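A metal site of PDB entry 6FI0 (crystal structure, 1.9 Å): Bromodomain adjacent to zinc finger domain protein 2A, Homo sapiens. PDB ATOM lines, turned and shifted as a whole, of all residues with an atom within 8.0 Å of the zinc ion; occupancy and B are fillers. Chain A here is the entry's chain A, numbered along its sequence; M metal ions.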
ATOM      1  N   THR A   8      21.698 -10.111   5.826  1.00  0.00           N
ATOM      2  CA  THR A   8      21.842  -9.906   4.376  1.00  0.00           C
ATOM      3  C   THR A   8      20.496  -9.555   3.741  1.00  0.00           C
ATOM      4  O   THR A   8      19.414  -9.783   4.317  1.00  0.00           O
ATOM      5  CB  THR A   8      22.450 -11.125   3.662  1.00  0.00           C
ATOM      6  OG1 THR A   8      21.661 -12.265   3.970  1.00  0.00           O
ATOM      7  CG2 THR A   8      23.911 -11.355   4.068  1.00  0.00           C
ATOM      8  N   CYS A   9      20.575  -9.008   2.550  1.00  0.00           N
ATOM      9  CA  CYS A   9      19.407  -8.606   1.781  1.00  0.00           C
ATOM     10  C   CYS A   9      18.754  -9.794   1.091  1.00  0.00           C
ATOM     11  O   CYS A   9      19.427 -10.529   0.356  1.00  0.00           O
ATOM     12  CB  CYS A   9      19.810  -7.558   0.746  1.00  0.00           C
ATOM     13  SG  CYS A   9      18.587  -7.046  -0.486  1.00  0.00           S
ATOM     14  N   LEU A  10      17.447  -9.926   1.271  1.00  0.00           N
ATOM     15  CA  LEU A  10      16.643 -10.967   0.636  1.00  0.00           C
ATOM     16  C   LEU A  10      16.722 -10.998  -0.904  1.00  0.00           C
ATOM     17  O   LEU A  10      16.717 -12.075  -1.491  1.00  0.00           O
ATOM     18  CB  LEU A  10      15.172 -10.898   1.068  1.00  0.00           C
ATOM     19  CG  LEU A  10      14.794 -11.406   2.447  1.00  0.00           C
ATOM     20  CD1 LEU A  10      13.371 -11.007   2.804  1.00  0.00           C
ATOM     21  CD2 LEU A  10      14.971 -12.940   2.560  1.00  0.00           C
ATOM     22  N   VAL A  11      16.815  -9.832  -1.544  1.00  0.00           N
ATOM     23  CA  VAL A  11      16.797  -9.703  -2.982  1.00  0.00           C
ATOM     24  C   VAL A  11      18.174  -9.982  -3.588  1.00  0.00           C
ATOM     25  O   VAL A  11      18.281 -10.841  -4.474  1.00  0.00           O
ATOM     26  CB  VAL A  11      16.302  -8.275  -3.410  1.00  0.00           C
ATOM     27  CG1 VAL A  11      16.371  -8.079  -4.916  1.00  0.00           C
ATOM     28  CG2 VAL A  11      14.885  -8.068  -2.891  1.00  0.00           C
ATOM     29  N   CYS A  12      19.212  -9.295  -3.120  1.00  0.00           N
ATOM     30  CA  CYS A  12      20.557  -9.404  -3.730  1.00  0.00           C
ATOM     31  C   CYS A  12      21.571 -10.258  -2.941  1.00  0.00           C
ATOM     32  O   CYS A  12      22.681 -10.498  -3.433  1.00  0.00           O
ATOM     33  CB  CYS A  12      21.144  -8.005  -3.954  1.00  0.00           C
ATOM     34  SG  CYS A  12      21.848  -7.245  -2.496  1.00  0.00           S
ATOM     35  N   ARG A  13      21.214 -10.652  -1.724  1.00  0.00           N
ATOM     36  CA  ARG A  13      22.057 -11.491  -0.840  1.00  0.00           C
ATOM     37  C   ARG A  13      23.382 -10.888  -0.337  1.00  0.00           C
ATOM     38  O   ARG A  13      24.189 -11.589   0.234  1.00  0.00           O
ATOM     39  CB  ARG A  13      22.261 -12.885  -1.455  1.00  0.00           C
ATOM     40  CG  ARG A  13      20.942 -13.594  -1.653  1.00  0.00           C
ATOM     41  CD  ARG A  13      21.137 -14.920  -2.326  1.00  0.00           C
ATOM     42  NE  ARG A  13      19.997 -15.794  -2.017  1.00  0.00           N
ATOM     43  CZ  ARG A  13      20.012 -17.128  -1.972  1.00  0.00           C
ATOM     44  NH1 ARG A  13      21.128 -17.831  -2.202  1.00  0.00           N
ATOM     45  NH2 ARG A  13      18.890 -17.786  -1.660  1.00  0.00           N
ATOM     46  N   LYS A  14      23.588  -9.598  -0.516  1.00  0.00           N
ATOM     47  CA  LYS A  14      24.768  -8.936   0.066  1.00  0.00           C
ATOM     48  C   LYS A  14      24.341  -8.272   1.371  1.00  0.00           C
ATOM     49  O   LYS A  14      23.148  -8.011   1.588  1.00  0.00           O
ATOM     50  CB  LYS A  14      25.327  -7.930  -0.901  1.00  0.00           C
ATOM     51  CG  LYS A  14      25.599  -8.528  -2.265  1.00  0.00           C
ATOM     52  CD  LYS A  14      26.097  -7.473  -3.234  1.00  0.00           C
ATOM     53  CE  LYS A  14      27.061  -8.066  -4.228  1.00  0.00           C
ATOM     54  NZ  LYS A  14      27.460  -7.080  -5.257  1.00  0.00           N
ATOM     55  N   GLY A  15      25.309  -8.091   2.261  1.00  0.00           N
ATOM     56  CA  GLY A  15      25.095  -7.426   3.544  1.00  0.00           C
ATOM     57  C   GLY A  15      25.845  -6.104   3.639  1.00  0.00           C
ATOM     58  O   GLY A  15      26.008  -5.585   4.740  1.00  0.00           O
ATOM     59  N   ASP A  16      26.260  -5.555   2.485  1.00  0.00           N
ATOM     60  CA  ASP A  16      26.974  -4.268   2.423  1.00  0.00           C
ATOM     61  C   ASP A  16      25.996  -3.080   2.432  1.00  0.00           C
ATOM     62  O   ASP A  16      24.772  -3.268   2.380  1.00  0.00           O
ATOM     63  CB  ASP A  16      27.907  -4.227   1.199  1.00  0.00           C
ATOM     64  CG  ASP A  16      27.170  -4.341  -0.124  1.00  0.00           C
ATOM     65  OD1 ASP A  16      25.951  -4.567  -0.158  1.00  0.00           O
ATOM     66  OD2 ASP A  16      27.846  -4.243  -1.165  1.00  0.00           O
ATOM     67  N   PHE A  20      21.708   1.360   4.404  1.00  0.00           N
ATOM     68  CA  PHE A  20      20.545   1.227   3.506  1.00  0.00           C
ATOM     69  C   PHE A  20      19.739  -0.055   3.724  1.00  0.00           C
ATOM     70  O   PHE A  20      18.796  -0.337   2.959  1.00  0.00           O
ATOM     71  CB  PHE A  20      21.024   1.273   2.034  1.00  0.00           C
ATOM     72  CG  PHE A  20      21.548   2.610   1.609  1.00  0.00           C
ATOM     73  CD1 PHE A  20      22.875   2.971   1.843  1.00  0.00           C
ATOM     74  CD2 PHE A  20      20.727   3.515   0.939  1.00  0.00           C
ATOM     75  CE1 PHE A  20      23.369   4.205   1.462  1.00  0.00           C
ATOM     76  CE2 PHE A  20      21.229   4.747   0.539  1.00  0.00           C
ATOM     77  CZ  PHE A  20      22.535   5.091   0.810  1.00  0.00           C
ATOM     78  N   LEU A  21      20.079  -0.806   4.760  1.00  0.00           N
ATOM     79  CA  LEU A  21      19.528  -2.131   4.948  1.00  0.00           C
ATOM     80  C   LEU A  21      18.338  -2.065   5.892  1.00  0.00           C
ATOM     81  O   LEU A  21      18.499  -1.671   7.042  1.00  0.00           O
ATOM     82  CB  LEU A  21      20.641  -3.008   5.497  1.00  0.00           C
ATOM     83  CG  LEU A  21      20.612  -4.492   5.439  1.00  0.00           C
ATOM     84  CD1 LEU A  21      20.199  -4.998   4.063  1.00  0.00           C
ATOM     85  CD2 LEU A  21      22.013  -4.991   5.796  1.00  0.00           C
ATOM     86  N   GLY A  30      16.461  -9.240   6.061  1.00  0.00           N
ATOM     87  CA  GLY A  30      16.753  -7.827   5.694  1.00  0.00           C
ATOM     88  C   GLY A  30      16.530  -7.516   4.247  1.00  0.00           C
ATOM     89  O   GLY A  30      16.288  -8.419   3.469  1.00  0.00           O
ATOM     90  N   CYS A  31      16.568  -6.231   3.855  1.00  0.00           N
ATOM     91  CA  CYS A  31      16.449  -5.880   2.429  1.00  0.00           C
ATOM     92  C   CYS A  31      16.984  -4.488   2.225  1.00  0.00           C
ATOM     93  O   CYS A  31      16.594  -3.590   2.972  1.00  0.00           O
ATOM     94  CB  CYS A  31      14.972  -5.915   2.027  1.00  0.00           C
ATOM     95  SG  CYS A  31      14.632  -5.640   0.273  1.00  0.00           S
ATOM     96  N   HIS A  32      17.861  -4.292   1.223  1.00  0.00           N
ATOM     97  CA  HIS A  32      18.323  -2.958   0.891  1.00  0.00           C
ATOM     98  C   HIS A  32      17.099  -2.173   0.458  1.00  0.00           C
ATOM     99  O   HIS A  32      16.299  -2.682  -0.333  1.00  0.00           O
ATOM    100  CB  HIS A  32      19.348  -2.948  -0.285  1.00  0.00           C
ATOM    101  CG  HIS A  32      20.643  -3.604   0.042  1.00  0.00           C
ATOM    102  ND1 HIS A  32      21.074  -4.775  -0.562  1.00  0.00           N
ATOM    103  CD2 HIS A  32      21.610  -3.245   0.930  1.00  0.00           C
ATOM    104  CE1 HIS A  32      22.250  -5.100  -0.055  1.00  0.00           C
ATOM    105  NE2 HIS A  32      22.597  -4.195   0.850  1.00  0.00           N
ATOM    106  N   ILE A  33      16.991  -0.937   0.894  1.00  0.00           N
ATOM    107  CA  ILE A  33      15.917  -0.084   0.378  1.00  0.00           C
ATOM    108  C   ILE A  33      15.969   0.047  -1.117  1.00  0.00           C
ATOM    109  O   ILE A  33      14.936   0.111  -1.756  1.00  0.00           O
ATOM    110  CB  ILE A  33      15.873   1.284   1.040  1.00  0.00           C
ATOM    111  CG1 ILE A  33      17.156   2.113   0.803  1.00  0.00           C
ATOM    112  CG2 ILE A  33      15.499   1.139   2.529  1.00  0.00           C
ATOM    113  CD1 ILE A  33      16.907   3.548   1.281  1.00  0.00           C
ATOM    114  N   TYR A  34      17.161   0.039  -1.689  1.00  0.00           N
ATOM    115  CA  TYR A  34      17.309   0.162  -3.137  1.00  0.00           C
ATOM    116  C   TYR A  34      16.994  -1.106  -3.914  1.00  0.00           C
ATOM    117  O   TYR A  34      16.861  -1.043  -5.164  1.00  0.00           O
ATOM    118  CB  TYR A  34      18.724   0.649  -3.523  1.00  0.00           C
ATOM    119  CG  TYR A  34      19.905  -0.042  -2.877  1.00  0.00           C
ATOM    120  CD1 TYR A  34      20.446  -1.215  -3.418  1.00  0.00           C
ATOM    121  CD2 TYR A  34      20.579   0.529  -1.787  1.00  0.00           C
ATOM    122  CE1 TYR A  34      21.581  -1.822  -2.861  1.00  0.00           C
ATOM    123  CE2 TYR A  34      21.728  -0.050  -1.260  1.00  0.00           C
ATOM    124  CZ  TYR A  34      22.207  -1.218  -1.764  1.00  0.00           C
ATOM    125  OH  TYR A  34      23.380  -1.784  -1.249  1.00  0.00           O
ATOM    126  N   CYS A  35      16.944  -2.236  -3.213  1.00  0.00           N
ATOM    127  CA  CYS A  35      16.506  -3.519  -3.801  1.00  0.00           C
ATOM    128  C   CYS A  35      15.009  -3.750  -3.765  1.00  0.00           C
ATOM    129  O   CYS A  35      14.485  -4.501  -4.561  1.00  0.00           O
ATOM    130  CB  CYS A  35      17.213  -4.679  -3.118  1.00  0.00           C
ATOM    131  SG  CYS A  35      18.983  -4.595  -3.463  1.00  0.00           S
ATOM    132  N   HIS A  36      14.340  -3.069  -2.865  1.00  0.00           N
ATOM    133  CA  HIS A  36      12.904  -3.180  -2.693  1.00  0.00           C
ATOM    134  C   HIS A  36      12.125  -2.652  -3.885  1.00  0.00           C
ATOM    135  O   HIS A  36      12.513  -1.627  -4.468  1.00  0.00           O
ATOM    136  CB  HIS A  36      12.504  -2.393  -1.469  1.00  0.00           C
ATOM    137  CG  HIS A  36      11.200  -2.795  -0.875  1.00  0.00           C
ATOM    138  ND1 HIS A  36       9.984  -2.276  -1.281  1.00  0.00           N
ATOM    139  CD2 HIS A  36      10.928  -3.646   0.152  1.00  0.00           C
ATOM    140  CE1 HIS A  36       9.031  -2.817  -0.549  1.00  0.00           C
ATOM    141  NE2 HIS A  36       9.569  -3.645   0.323  1.00  0.00           N
HETATM  142 ZN    ZN M   1      20.060  -5.845  -1.826  1.00  0.00          ZN
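A ring nitrogen (NE2) of His 32 sits close to the side-chain hydroxyl (OH) of Tyr 34 (3.3 Å). The backbone carbonyl oxygen (O) of Asp 16 sits at hydrogen-bond distance from a ring nitrogen (NE2) of His 32 (2.8 Å). SG of Cys 9 lies close to N of Val 11. The backbone NH (N) of Cys 9 is in hydrogen-bond range of the backbone carbonyl oxygen (O) of Lys 14 (2.9 Å). The backbone NH (N) of Lys 14 lies close to the side-chain sulfur (SG) of Cys 12, at 3.5 Å.
The nearest printed residue that does not touch the zinc ion is Tyr 34 (4.4 Å).
The zinc ion is bound by a ring nitrogen (ND1) of His 32 (1.9 Å), the side-chain sulfur of Cys 35 (2.3 Å), the side-chain sulfur of Cys 9 (2.3 Å) and the side-chain sulfur of Cys 12 (2.4 Å). The zinc ion has four donor atoms within binding distance.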
